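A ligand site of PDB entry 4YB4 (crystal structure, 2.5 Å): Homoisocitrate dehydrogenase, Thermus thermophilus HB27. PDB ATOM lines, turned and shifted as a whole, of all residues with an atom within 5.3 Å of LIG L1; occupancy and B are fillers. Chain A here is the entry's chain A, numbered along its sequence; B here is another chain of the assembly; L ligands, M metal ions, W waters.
ND2 of Asn 273 lies within hydrogen-bond range of OD2 of Asp 313, 2.9 Å away.
NH2 of Arg 88 is in salt-bridge range of OE2 of Glu 257.
OG of Ser 262 is in hydrogen-bond range of OG1 of Thr 71, 2.8 Å away.
The backbone NH (N) of Ile 13 sits at hydrogen-bond distance from the backbone carbonyl oxygen (O) of Ser 262, at 2.8 Å.
A ring nitrogen (ND1) of His 260 is in hydrogen-bond range of the backbone carbonyl oxygen (O) of Leu 241.
The side-chain amide oxygen (OD1) of Asn 205 of chain B is in hydrogen-bond range of the side-chain amide nitrogen (NE2) of Gln 209 of chain B, 3.0 Å away.
An oxygen (O13) of LIG L1 sits at hydrogen-bond distance from an oxygen (O6) of LG2 L2 (2.8 Å).
Water W2 lies within hydrogen-bond range of O9 of LIG L1 (2.5 Å), ND2 of Asn 205 of chain B (2.9 Å) and N of Ile 202 of chain B (2.9 Å).
Water W3 bridges O9 of LIG L1 and OD1 of Asp 204 of chain B.
Water W10 lies within hydrogen-bond range of an oxygen (O14) of LIG L1 and the backbone NH (N) of Ile 84.
Water W7 bridges an oxygen (O5) of LIG L1 (2.9 Å) and the side-chain amide nitrogen (NE2) of Gln 209 of chain B (3.1 Å).
Water W8 lies within hydrogen-bond range of O5 of LIG L1 (3.0 Å), NE2 of Gln 209 of chain B (3.2 Å) and ND2 of Asn 205 of chain B (3.3 Å).
Water W9 lies within hydrogen-bond range of the side-chain carboxylate of Asp 313 (2.6 Å) and the backbone carbonyl oxygen of Ile 271 (2.7 Å).
Residues that only touch LIG L1: Ile 13 (3.6 Å), Phe 67 (3.6 Å), Ala 69 (3.6 Å), Thr 71 (3.6 Å), Ile 84 (3.8 Å), Leu 241 (3.6 Å), Gly 242 (3.8 Å), Val 259 (3.8 Å), Pro 264 (3.7 Å), Ile 266 (3.5 Å), Ala 272 (3.9 Å), Asp 313 (3.8 Å), Ile 202 of chain B (3.5 Å), Asn 205 of chain B (3.3 Å) and Met 208 of chain B (3.7 Å).
Hydrophobic or aromatic side chains within 4 Å of LIG L1: Ile 13, Phe 67, Ile 84, Leu 241, His 260, Ala 263, Pro 264, Ile 266, Ile 202 of chain B and Met 208 of chain B.
The nearest printed residue that does not touch LIG L1 is Gln 209 of chain B (4.04 Å).
N of Ser 262 lies within hydrogen-bond range of O11 of LIG L1.
The backbone carbonyl oxygen (O) of Ser 72 sits at hydrogen-bond distance from an oxygen (O12) of LIG L1 (3.3 Å).
The backbone carbonyl oxygen of Asn 273 sits at hydrogen-bond distance from a nitrogen (N3) of LIG L1 (2.9 Å).
An oxygen (O6) of LG2 L2 lies within hydrogen-bond range of the side-chain amide nitrogen (ND2) of Asn 173 of chain B (2.9 Å).
The side-chain hydroxyl (OG) of Ser 262 lies close to an oxygen (O11) of LIG L1, 3.4 Å away.
The backbone NH (N) of Ala 263 is in hydrogen-bond range of an oxygen (O2) of LIG L1 (2.8 Å).
OG of Ser 72 is in hydrogen-bond range of O13 of LIG L1 (2.9 Å).
N of Ala 70 sits at hydrogen-bond distance from O14 of LIG L1 (2.9 Å).
The side-chain carboxylate (OD1) of Asp 265 sits at hydrogen-bond distance from an oxygen (O6) of LIG L1 (2.6 Å).
The guanidinium group (NH1) of Arg 88 lies within salt-bridge range of an oxygen (O4) of LG2 L2.
OG of Ser 72 lies within hydrogen-bond range of O6 of LG2 L2 (2.7 Å).
ND2 of Asn 173 of chain B sits at hydrogen-bond distance from O13 of LIG L1, 3.2 Å away.
A nitrogen (N4) of LIG L1 lies within hydrogen-bond range of the backbone NH (N) of Asn 273, at 3.0 Å.
O1 of LIG L1 lies within hydrogen-bond range of N of Gly 261 (2.7 Å).
The backbone NH (N) of Ser 72 is in hydrogen-bond range of an oxygen (O12) of LIG L1 (3.1 Å).
OE1 of Glu 257 lies within hydrogen-bond range of N7 of LIG L1 (2.7 Å).
ND1 of His 260 sits close to N3 of LIG L1, at 3.5 Å.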
ATOM      1  N   ILE A  13      -7.976   2.887   3.193  1.00  0.00           N
ATOM      2  CA  ILE A  13      -8.076   4.322   2.872  1.00  0.00           C
ATOM      3  C   ILE A  13      -6.738   5.085   2.938  1.00  0.00           C
ATOM      4  O   ILE A  13      -6.690   6.254   2.592  1.00  0.00           O
ATOM      5  CB  ILE A  13      -9.126   5.059   3.732  1.00  0.00           C
ATOM      6  CG1 ILE A  13      -8.760   5.027   5.218  1.00  0.00           C
ATOM      7  CG2 ILE A  13     -10.507   4.483   3.492  1.00  0.00           C
ATOM      8  CD1 ILE A  13      -9.537   6.016   6.043  1.00  0.00           C
ATOM      9  N   VAL A  17      -6.028   8.817   1.268  1.00  0.00           N
ATOM     10  CA  VAL A  17      -5.741  10.020   2.070  1.00  0.00           C
ATOM     11  C   VAL A  17      -4.278  10.482   2.020  1.00  0.00           C
ATOM     12  O   VAL A  17      -4.000  11.673   2.204  1.00  0.00           O
ATOM     13  CB  VAL A  17      -6.219   9.892   3.551  1.00  0.00           C
ATOM     14  CG1 VAL A  17      -7.669   9.450   3.608  1.00  0.00           C
ATOM     15  CG2 VAL A  17      -5.339   8.945   4.364  1.00  0.00           C
ATOM     16  N   PHE A  67       2.602   8.596   7.226  1.00  0.00           N
ATOM     17  CA  PHE A  67       2.124   7.246   7.153  1.00  0.00           C
ATOM     18  C   PHE A  67       0.633   7.199   7.015  1.00  0.00           C
ATOM     19  O   PHE A  67      -0.056   7.962   7.587  1.00  0.00           O
ATOM     20  CB  PHE A  67       2.505   6.549   8.428  1.00  0.00           C
ATOM     21  CG  PHE A  67       2.116   5.119   8.495  1.00  0.00           C
ATOM     22  CD1 PHE A  67       2.963   4.161   8.030  1.00  0.00           C
ATOM     23  CD2 PHE A  67       0.950   4.733   9.072  1.00  0.00           C
ATOM     24  CE1 PHE A  67       2.629   2.833   8.101  1.00  0.00           C
ATOM     25  CE2 PHE A  67       0.612   3.426   9.135  1.00  0.00           C
ATOM     26  CZ  PHE A  67       1.443   2.469   8.655  1.00  0.00           C
ATOM     27  N   GLY A  68       0.145   6.238   6.253  1.00  0.00           N
ATOM     28  CA  GLY A  68      -1.266   6.104   6.032  1.00  0.00           C
ATOM     29  C   GLY A  68      -2.008   5.383   7.109  1.00  0.00           C
ATOM     30  O   GLY A  68      -2.563   5.989   7.963  1.00  0.00           O
ATOM     31  N   ALA A  69      -2.033   4.073   7.021  1.00  0.00           N
ATOM     32  CA  ALA A  69      -2.629   3.223   8.009  1.00  0.00           C
ATOM     33  C   ALA A  69      -2.450   1.843   7.476  1.00  0.00           C
ATOM     34  O   ALA A  69      -2.361   1.670   6.307  1.00  0.00           O
ATOM     35  CB  ALA A  69      -4.087   3.515   8.172  1.00  0.00           C
ATOM     36  N   ALA A  70      -2.355   0.859   8.344  1.00  0.00           N
ATOM     37  CA  ALA A  70      -2.191  -0.504   7.909  1.00  0.00           C
ATOM     38  C   ALA A  70      -3.096  -1.461   8.634  1.00  0.00           C
ATOM     39  O   ALA A  70      -3.349  -1.315   9.794  1.00  0.00           O
ATOM     40  CB  ALA A  70      -0.760  -0.904   8.072  1.00  0.00           C
ATOM     41  N   THR A  71      -3.593  -2.441   7.918  1.00  0.00           N
ATOM     42  CA  THR A  71      -4.452  -3.445   8.454  1.00  0.00           C
ATOM     43  C   THR A  71      -3.722  -4.500   9.255  1.00  0.00           C
ATOM     44  O   THR A  71      -2.667  -4.913   8.918  1.00  0.00           O
ATOM     45  CB  THR A  71      -5.221  -4.147   7.334  1.00  0.00           C
ATOM     46  OG1 THR A  71      -5.996  -3.193   6.640  1.00  0.00           O
ATOM     47  CG2 THR A  71      -6.108  -5.187   7.864  1.00  0.00           C
ATOM     48  N   SER A  72      -4.332  -4.955  10.313  1.00  0.00           N
ATOM     49  CA  SER A  72      -3.770  -6.067  11.060  1.00  0.00           C
ATOM     50  C   SER A  72      -4.885  -7.027  11.449  1.00  0.00           C
ATOM     51  O   SER A  72      -6.013  -6.609  11.714  1.00  0.00           O
ATOM     52  CB  SER A  72      -3.011  -5.583  12.288  1.00  0.00           C
ATOM     53  OG  SER A  72      -3.880  -4.890  13.149  1.00  0.00           O
ATOM     54  N   ILE A  84       2.842  -0.278  12.119  1.00  0.00           N
ATOM     55  CA  ILE A  84       3.106   0.975  12.825  1.00  0.00           C
ATOM     56  C   ILE A  84       3.680   0.682  14.203  1.00  0.00           C
ATOM     57  O   ILE A  84       4.558   1.381  14.675  1.00  0.00           O
ATOM     58  CB  ILE A  84       1.846   1.887  12.920  1.00  0.00           C
ATOM     59  CG1 ILE A  84       2.225   3.304  13.335  1.00  0.00           C
ATOM     60  CG2 ILE A  84       0.825   1.341  13.921  1.00  0.00           C
ATOM     61  CD1 ILE A  84       2.968   4.079  12.264  1.00  0.00           C
ATOM     62  N   ARG A  88       7.117   2.119  15.641  1.00  0.00           N
ATOM     63  CA  ARG A  88       7.124   2.818  16.939  1.00  0.00           C
ATOM     64  C   ARG A  88       8.220   2.304  17.873  1.00  0.00           C
ATOM     65  O   ARG A  88       8.983   3.093  18.441  1.00  0.00           O
ATOM     66  CB  ARG A  88       5.761   2.689  17.627  1.00  0.00           C
ATOM     67  CG  ARG A  88       4.657   3.538  17.017  1.00  0.00           C
ATOM     68  CD  ARG A  88       3.300   3.222  17.645  1.00  0.00           C
ATOM     69  NE  ARG A  88       2.264   3.950  16.927  1.00  0.00           N
ATOM     70  CZ  ARG A  88       0.958   3.711  16.987  1.00  0.00           C
ATOM     71  NH1 ARG A  88       0.463   2.788  17.797  1.00  0.00           N
ATOM     72  NH2 ARG A  88       0.133   4.418  16.228  1.00  0.00           N
ATOM     73  N   LEU A 241     -13.056  10.485  13.429  1.00  0.00           N
ATOM     74  CA  LEU A 241     -11.757  10.030  12.958  1.00  0.00           C
ATOM     75  C   LEU A 241     -11.398  10.550  11.576  1.00  0.00           C
ATOM     76  O   LEU A 241     -10.256  10.444  11.154  1.00  0.00           O
ATOM     77  CB  LEU A 241     -11.696   8.510  12.953  1.00  0.00           C
ATOM     78  CG  LEU A 241     -11.615   7.828  14.315  1.00  0.00           C
ATOM     79  CD1 LEU A 241     -11.673   6.313  14.175  1.00  0.00           C
ATOM     80  CD2 LEU A 241     -10.334   8.236  15.033  1.00  0.00           C
ATOM     81  N   GLY A 242     -12.364  11.130  10.865  1.00  0.00           N
ATOM     82  CA  GLY A 242     -12.077  11.832   9.615  1.00  0.00           C
ATOM     83  C   GLY A 242     -11.140  13.007   9.772  1.00  0.00           C
ATOM     84  O   GLY A 242     -10.529  13.450   8.804  1.00  0.00           O
ATOM     85  N   GLU A 257       0.869  10.528  11.194  1.00  0.00           N
ATOM     86  CA  GLU A 257      -0.189   9.662  10.689  1.00  0.00           C
ATOM     87  C   GLU A 257      -1.517  10.039  11.338  1.00  0.00           C
ATOM     88  O   GLU A 257      -1.562  10.502  12.482  1.00  0.00           O
ATOM     89  CB  GLU A 257       0.107   8.175  10.997  1.00  0.00           C
ATOM     90  CG  GLU A 257       0.008   7.820  12.463  1.00  0.00           C
ATOM     91  CD  GLU A 257       0.183   6.343  12.751  1.00  0.00           C
ATOM     92  OE1 GLU A 257      -0.194   5.522  11.907  1.00  0.00           O
ATOM     93  OE2 GLU A 257       0.689   5.996  13.851  1.00  0.00           O
ATOM     94  N   PRO A 258      -2.616   9.826  10.592  1.00  0.00           N
ATOM     95  CA  PRO A 258      -3.937   9.967  11.207  1.00  0.00           C
ATOM     96  C   PRO A 258      -4.075   9.018  12.375  1.00  0.00           C
ATOM     97  O   PRO A 258      -3.446   7.954  12.406  1.00  0.00           O
ATOM     98  CB  PRO A 258      -4.897   9.521  10.105  1.00  0.00           C
ATOM     99  CG  PRO A 258      -4.129   9.557   8.836  1.00  0.00           C
ATOM    100  CD  PRO A 258      -2.663   9.444   9.177  1.00  0.00           C
ATOM    101  N   VAL A 259      -4.936   9.370  13.300  1.00  0.00           N
ATOM    102  CA  VAL A 259      -5.355   8.435  14.345  1.00  0.00           C
ATOM    103  C   VAL A 259      -6.085   7.226  13.763  1.00  0.00           C
ATOM    104  O   VAL A 259      -6.010   6.123  14.320  1.00  0.00           O
ATOM    105  CB  VAL A 259      -6.233   9.170  15.374  1.00  0.00           C
ATOM    106  CG1 VAL A 259      -6.844   8.207  16.362  1.00  0.00           C
ATOM    107  CG2 VAL A 259      -5.403  10.210  16.095  1.00  0.00           C
ATOM    108  N   HIS A 260      -6.763   7.407  12.641  1.00  0.00           N
ATOM    109  CA  HIS A 260      -7.601   6.340  12.067  1.00  0.00           C
ATOM    110  C   HIS A 260      -6.828   5.202  11.425  1.00  0.00           C
ATOM    111  O   HIS A 260      -5.656   5.335  11.055  1.00  0.00           O
ATOM    112  CB  HIS A 260      -8.632   6.904  11.067  1.00  0.00           C
ATOM    113  CG  HIS A 260      -8.058   7.425   9.788  1.00  0.00           C
ATOM    114  ND1 HIS A 260      -8.148   8.749   9.417  1.00  0.00           N
ATOM    115  CD2 HIS A 260      -7.406   6.794   8.772  1.00  0.00           C
ATOM    116  CE1 HIS A 260      -7.578   8.919   8.234  1.00  0.00           C
ATOM    117  NE2 HIS A 260      -7.111   7.749   7.831  1.00  0.00           N
ATOM    118  N   GLY A 261      -7.511   4.082  11.287  1.00  0.00           N
ATOM    119  CA  GLY A 261      -6.982   2.887  10.628  1.00  0.00           C
ATOM    120  C   GLY A 261      -7.314   2.859   9.158  1.00  0.00           C
ATOM    121  O   GLY A 261      -7.627   3.896   8.555  1.00  0.00           O
ATOM    122  N   SER A 262      -7.263   1.658   8.583  1.00  0.00           N
ATOM    123  CA  SER A 262      -7.404   1.484   7.147  1.00  0.00           C
ATOM    124  C   SER A 262      -8.861   1.575   6.686  1.00  0.00           C
ATOM    125  O   SER A 262      -9.110   1.661   5.489  1.00  0.00           O
ATOM    126  CB  SER A 262      -6.788   0.145   6.723  1.00  0.00           C
ATOM    127  OG  SER A 262      -7.317  -0.887   7.526  1.00  0.00           O
ATOM    128  N   ALA A 263      -9.795   1.546   7.625  1.00  0.00           N
ATOM    129  CA  ALA A 263     -11.216   1.783   7.374  1.00  0.00           C
ATOM    130  C   ALA A 263     -11.743   0.924   6.219  1.00  0.00           C
ATOM    131  O   ALA A 263     -12.192   1.446   5.207  1.00  0.00           O
ATOM    132  CB  ALA A 263     -11.460   3.262   7.102  1.00  0.00           C
ATOM    133  N   PRO A 264     -11.687  -0.406   6.380  1.00  0.00           N
ATOM    134  CA  PRO A 264     -12.076  -1.328   5.319  1.00  0.00           C
ATOM    135  C   PRO A 264     -13.536  -1.234   4.910  1.00  0.00           C
ATOM    136  O   PRO A 264     -13.903  -1.716   3.837  1.00  0.00           O
ATOM    137  CB  PRO A 264     -11.828  -2.719   5.929  1.00  0.00           C
ATOM    138  CG  PRO A 264     -11.143  -2.494   7.239  1.00  0.00           C
ATOM    139  CD  PRO A 264     -11.457  -1.098   7.662  1.00  0.00           C
ATOM    140  N   ASP A 265     -14.381  -0.650   5.747  1.00  0.00           N
ATOM    141  CA  ASP A 265     -15.788  -0.500   5.419  1.00  0.00           C
ATOM    142  C   ASP A 265     -16.016   0.538   4.289  1.00  0.00           C
ATOM    143  O   ASP A 265     -16.982   0.422   3.534  1.00  0.00           O
ATOM    144  CB  ASP A 265     -16.619  -0.217   6.683  1.00  0.00           C
ATOM    145  CG  ASP A 265     -16.180   1.039   7.450  1.00  0.00           C
ATOM    146  OD1 ASP A 265     -15.066   1.579   7.232  1.00  0.00           O
ATOM    147  OD2 ASP A 265     -16.978   1.472   8.300  1.00  0.00           O
ATOM    148  N   ILE A 266     -15.120   1.516   4.145  1.00  0.00           N
ATOM    149  CA  ILE A 266     -15.234   2.522   3.073  1.00  0.00           C
ATOM    150  C   ILE A 266     -14.027   2.576   2.136  1.00  0.00           C
ATOM    151  O   ILE A 266     -13.960   3.440   1.246  1.00  0.00           O
ATOM    152  CB  ILE A 266     -15.459   3.964   3.630  1.00  0.00           C
ATOM    153  CG1 ILE A 266     -14.210   4.466   4.387  1.00  0.00           C
ATOM    154  CG2 ILE A 266     -16.717   4.018   4.501  1.00  0.00           C
ATOM    155  CD1 ILE A 266     -14.343   5.863   4.958  1.00  0.00           C
ATOM    156  N   ILE A 271     -14.379   8.119  -0.878  1.00  0.00           N
ATOM    157  CA  ILE A 271     -15.092   9.077  -0.007  1.00  0.00           C
ATOM    158  C   ILE A 271     -14.405   9.382   1.322  1.00  0.00           C
ATOM    159  O   ILE A 271     -14.868  10.250   2.043  1.00  0.00           O
ATOM    160  CB  ILE A 271     -16.551   8.646   0.269  1.00  0.00           C
ATOM    161  CG1 ILE A 271     -16.613   7.273   0.963  1.00  0.00           C
ATOM    162  CG2 ILE A 271     -17.345   8.620  -1.020  1.00  0.00           C
ATOM    163  CD1 ILE A 271     -18.009   6.885   1.412  1.00  0.00           C
ATOM    164  N   ALA A 272     -13.321   8.676   1.649  1.00  0.00           N
ATOM    165  CA  ALA A 272     -12.664   8.911   2.918  1.00  0.00           C
ATOM    166  C   ALA A 272     -12.312  10.368   3.101  1.00  0.00           C
ATOM    167  O   ALA A 272     -11.870  11.029   2.155  1.00  0.00           O
ATOM    168  CB  ALA A 272     -11.414   8.065   3.047  1.00  0.00           C
ATOM    169  N   ASN A 273     -12.533  10.877   4.297  1.00  0.00           N
ATOM    170  CA  ASN A 273     -12.141  12.234   4.659  1.00  0.00           C
ATOM    171  C   ASN A 273     -10.618  12.266   4.819  1.00  0.00           C
ATOM    172  O   ASN A 273     -10.064  11.538   5.640  1.00  0.00           O
ATOM    173  CB  ASN A 273     -12.818  12.630   5.966  1.00  0.00           C
ATOM    174  CG  ASN A 273     -12.675  14.096   6.280  1.00  0.00           C
ATOM    175  OD1 ASN A 273     -11.830  14.803   5.736  1.00  0.00           O
ATOM    176  ND2 ASN A 273     -13.523  14.579   7.190  1.00  0.00           N
ATOM    177  N   PRO A 274      -9.944  13.093   4.016  1.00  0.00           N
ATOM    178  CA  PRO A 274      -8.490  13.222   4.088  1.00  0.00           C
ATOM    179  C   PRO A 274      -7.989  14.266   5.084  1.00  0.00           C
ATOM    180  O   PRO A 274      -6.800  14.544   5.124  1.00  0.00           O
ATOM    181  CB  PRO A 274      -8.144  13.683   2.667  1.00  0.00           C
ATOM    182  CG  PRO A 274      -9.268  14.601   2.320  1.00  0.00           C
ATOM    183  CD  PRO A 274     -10.498  13.942   2.933  1.00  0.00           C
ATOM    184  N   ASP A 313     -18.892  11.374   6.017  1.00  0.00           N
ATOM    185  CA  ASP A 313     -18.695  11.354   7.471  1.00  0.00           C
ATOM    186  C   ASP A 313     -19.062  12.693   8.134  1.00  0.00           C
ATOM    187  O   ASP A 313     -19.422  12.726   9.315  1.00  0.00           O
ATOM    188  CB  ASP A 313     -17.255  10.979   7.800  1.00  0.00           C
ATOM    189  CG  ASP A 313     -16.258  11.950   7.210  1.00  0.00           C
ATOM    190  OD1 ASP A 313     -16.149  11.946   5.962  1.00  0.00           O
ATOM    191  OD2 ASP A 313     -15.609  12.704   7.986  1.00  0.00           O
ATOM    192  N   ASN B 173      -6.257  -7.322  17.871  1.00  0.00           N
ATOM    193  CA  ASN B 173      -5.296  -6.802  16.906  1.00  0.00           C
ATOM    194  C   ASN B 173      -3.910  -6.549  17.513  1.00  0.00           C
ATOM    195  O   ASN B 173      -2.913  -6.910  16.912  1.00  0.00           O
ATOM    196  CB  ASN B 173      -5.867  -5.558  16.117  1.00  0.00           C
ATOM    197  CG  ASN B 173      -6.263  -4.333  17.033  1.00  0.00           C
ATOM    198  OD1 ASN B 173      -6.741  -4.489  18.169  1.00  0.00           O
ATOM    199  ND2 ASN B 173      -6.110  -3.115  16.483  1.00  0.00           N
ATOM    200  N   ILE B 202     -13.150  -3.185  17.500  1.00  0.00           N
ATOM    201  CA  ILE B 202     -11.937  -2.828  18.229  1.00  0.00           C
ATOM    202  C   ILE B 202     -12.308  -1.755  19.261  1.00  0.00           C
ATOM    203  O   ILE B 202     -13.098  -0.854  18.964  1.00  0.00           O
ATOM    204  CB  ILE B 202     -10.829  -2.366  17.262  1.00  0.00           C
ATOM    205  CG1 ILE B 202     -10.579  -3.453  16.195  1.00  0.00           C
ATOM    206  CG2 ILE B 202      -9.537  -2.120  18.032  1.00  0.00           C
ATOM    207  CD1 ILE B 202      -9.394  -3.183  15.284  1.00  0.00           C
ATOM    208  N   ASP B 204     -11.057   0.942  20.837  1.00  0.00           N
ATOM    209  CA  ASP B 204     -10.901   2.393  20.602  1.00  0.00           C
ATOM    210  C   ASP B 204     -11.991   2.926  19.663  1.00  0.00           C
ATOM    211  O   ASP B 204     -12.603   3.962  19.944  1.00  0.00           O
ATOM    212  CB  ASP B 204      -9.485   2.778  20.116  1.00  0.00           C
ATOM    213  CG  ASP B 204      -9.024   2.003  18.874  1.00  0.00           C
ATOM    214  OD1 ASP B 204      -9.664   1.002  18.475  1.00  0.00           O
ATOM    215  OD2 ASP B 204      -7.985   2.409  18.305  1.00  0.00           O
ATOM    216  N   ASN B 205     -12.227   2.207  18.575  1.00  0.00           N
ATOM    217  CA  ASN B 205     -13.315   2.510  17.664  1.00  0.00           C
ATOM    218  C   ASN B 205     -14.635   2.482  18.427  1.00  0.00           C
ATOM    219  O   ASN B 205     -15.471   3.352  18.258  1.00  0.00           O
ATOM    220  CB  ASN B 205     -13.344   1.467  16.562  1.00  0.00           C
ATOM    221  CG  ASN B 205     -14.429   1.718  15.528  1.00  0.00           C
ATOM    222  OD1 ASN B 205     -14.850   2.852  15.288  1.00  0.00           O
ATOM    223  ND2 ASN B 205     -14.861   0.650  14.886  1.00  0.00           N
ATOM    224  N   MET B 208     -15.079   5.677  20.187  1.00  0.00           N
ATOM    225  CA  MET B 208     -15.532   6.720  19.240  1.00  0.00           C
ATOM    226  C   MET B 208     -17.016   6.558  18.850  1.00  0.00           C
ATOM    227  O   MET B 208     -17.748   7.550  18.786  1.00  0.00           O
ATOM    228  CB  MET B 208     -14.631   6.777  18.007  1.00  0.00           C
ATOM    229  CG  MET B 208     -15.011   7.856  16.991  1.00  0.00           C
ATOM    230  SD  MET B 208     -16.295   7.278  15.864  1.00  0.00           S
ATOM    231  CE  MET B 208     -15.358   6.115  14.872  1.00  0.00           C
ATOM    232  N   GLN B 209     -17.476   5.331  18.637  1.00  0.00           N
ATOM    233  CA  GLN B 209     -18.861   5.114  18.233  1.00  0.00           C
ATOM    234  C   GLN B 209     -19.827   5.442  19.376  1.00  0.00           C
ATOM    235  O   GLN B 209     -20.931   5.950  19.138  1.00  0.00           O
ATOM    236  CB  GLN B 209     -19.098   3.667  17.784  1.00  0.00           C
ATOM    237  CG  GLN B 209     -18.225   3.162  16.630  1.00  0.00           C
ATOM    238  CD  GLN B 209     -18.524   3.821  15.300  1.00  0.00           C
ATOM    239  OE1 GLN B 209     -19.549   4.468  15.123  1.00  0.00           O
ATOM    240  NE2 GLN B 209     -17.618   3.648  14.331  1.00  0.00           N
HETATM  241  P1  LIG L   1     -10.805   2.603  11.641  1.00  0.00           P
HETATM  242  O1  LIG L   1     -10.051   3.729  12.221  1.00  0.00           O
HETATM  243  O2  LIG L   1     -10.170   2.215  10.268  1.00  0.00           O
HETATM  244  O3  LIG L   1     -12.313   3.071  11.396  1.00  0.00           O
HETATM  245  C1  LIG L   1     -13.270   3.115  12.436  1.00  0.00           C
HETATM  246  C2  LIG L   1     -14.477   3.807  11.796  1.00  0.00           C
HETATM  247  O4  LIG L   1     -14.125   5.185  11.457  1.00  0.00           O
HETATM  248  C3  LIG L   1     -14.848   3.101  10.491  1.00  0.00           C
HETATM  249  O5  LIG L   1     -16.245   2.917  10.396  1.00  0.00           O
HETATM  250  C4  LIG L   1     -14.328   4.047   9.402  1.00  0.00           C
HETATM  251  O6  LIG L   1     -15.125   3.945   8.242  1.00  0.00           O
HETATM  252  C5  LIG L   1     -14.393   5.420  10.050  1.00  0.00           C
HETATM  253  N1  LIG L   1     -13.285   6.264   9.523  1.00  0.00           N
HETATM  254  C6  LIG L   1     -12.002   6.172   9.848  1.00  0.00           C
HETATM  255  N2  LIG L   1     -11.300   7.041   9.124  1.00  0.00           N
HETATM  256  C7  LIG L   1     -12.163   7.691   8.341  1.00  0.00           C
HETATM  257  C8  LIG L   1     -12.007   8.684   7.432  1.00  0.00           C
HETATM  258  N3  LIG L   1     -10.792   9.163   7.224  1.00  0.00           N
HETATM  259  N4  LIG L   1     -13.048   9.179   6.762  1.00  0.00           N
HETATM  260  C9  LIG L   1     -14.310   8.650   7.017  1.00  0.00           C
HETATM  261  N5  LIG L   1     -14.454   7.648   7.953  1.00  0.00           N
HETATM  262  C10 LIG L   1     -13.386   7.193   8.596  1.00  0.00           C
HETATM  263  O7  LIG L   1     -10.639   1.474  12.763  1.00  0.00           O
HETATM  264  P2  LIG L   1     -11.035  -0.022  12.764  1.00  0.00           P
HETATM  265  O8  LIG L   1     -12.265  -0.160  11.804  1.00  0.00           O
HETATM  266  O9  LIG L   1     -11.291  -0.522  14.141  1.00  0.00           O
HETATM  267  O10 LIG L   1      -9.826  -0.912  12.147  1.00  0.00           O
HETATM  268  C11 LIG L   1      -9.425  -0.873  10.782  1.00  0.00           C
HETATM  269  C12 LIG L   1      -8.049  -1.475  10.652  1.00  0.00           C
HETATM  270  O11 LIG L   1      -7.044  -0.463  10.843  1.00  0.00           O
HETATM  271  C13 LIG L   1      -7.734  -2.554  11.675  1.00  0.00           C
HETATM  272  O12 LIG L   1      -7.047  -3.565  10.954  1.00  0.00           O
HETATM  273  C14 LIG L   1      -6.806  -1.904  12.687  1.00  0.00           C
HETATM  274  O13 LIG L   1      -5.943  -2.914  13.259  1.00  0.00           O
HETATM  275  C15 LIG L   1      -6.051  -0.955  11.780  1.00  0.00           C
HETATM  276  N6  LIG L   1      -5.533   0.311  12.327  1.00  0.00           N
HETATM  277  C16 LIG L   1      -4.293   0.753  11.901  1.00  0.00           C
HETATM  278  C17 LIG L   1      -3.731   1.959  12.294  1.00  0.00           C
HETATM  279  C18 LIG L   1      -2.440   2.315  11.842  1.00  0.00           C
HETATM  280  O14 LIG L   1      -1.754   1.585  11.131  1.00  0.00           O
HETATM  281  N7  LIG L   1      -1.937   3.480  12.256  1.00  0.00           N
HETATM  282  C19 LIG L   1      -4.492   2.835  13.115  1.00  0.00           C
HETATM  283  C20 LIG L   1      -5.768   2.374  13.506  1.00  0.00           C
HETATM  284  C21 LIG L   1      -6.295   1.150  13.126  1.00  0.00           C
HETATM  285  O1  LG2 L   2      -2.616   3.752  16.513  1.00  0.00           O
HETATM  286  C1  LG2 L   2      -3.741   3.429  16.865  1.00  0.00           C
HETATM  287  O2  LG2 L   2      -4.476   4.146  17.548  1.00  0.00           O
HETATM  288  C2  LG2 L   2      -4.267   2.020  16.477  1.00  0.00           C
HETATM  289  O3  LG2 L   2      -5.439   1.700  17.236  1.00  0.00           O
HETATM  290  C3  LG2 L   2      -3.154   0.966  16.724  1.00  0.00           C
HETATM  291  C4  LG2 L   2      -2.804   1.017  18.224  1.00  0.00           C
HETATM  292  O4  LG2 L   2      -1.998   1.921  18.563  1.00  0.00           O
HETATM  293  O5  LG2 L   2      -3.383   0.213  18.978  1.00  0.00           O
HETATM  294  C5  LG2 L   2      -3.606  -0.425  16.284  1.00  0.00           C
HETATM  295  C6  LG2 L   2      -2.304  -1.140  15.850  1.00  0.00           C
HETATM  296  C7  LG2 L   2      -2.516  -2.561  15.270  1.00  0.00           C
HETATM  297  O6  LG2 L   2      -3.675  -2.918  14.929  1.00  0.00           O
HETATM  298  O7  LG2 L   2      -1.486  -3.263  15.176  1.00  0.00           O
HETATM  299 MG    MG M   1      -6.380   3.570  18.225  1.00  0.00          MG
HETATM  300  O   HOH W   1      -9.524   3.395  15.101  1.00  0.00           O
HETATM  301  O   HOH W   2     -13.325  -1.787  14.957  1.00  0.00           O
HETATM  302  O   HOH W   3      -9.431   0.777  15.621  1.00  0.00           O
HETATM  303  O   HOH W   4     -17.035   6.769   7.550  1.00  0.00           O
HETATM  304  O   HOH W   5      -2.795   5.751  10.808  1.00  0.00           O
HETATM  305  O   HOH W   6      -2.584   5.465  14.167  1.00  0.00           O
HETATM  306  O   HOH W   7     -17.924   5.040  11.544  1.00  0.00           O
HETATM  307  O   HOH W   8     -17.176   1.009  12.518  1.00  0.00           O
HETATM  308  O   HOH W   9     -16.180   9.916   4.347  1.00  0.00           O
HETATM  309  O   HOH W  10      -0.257  -0.628  11.648  1.00  0.00           O
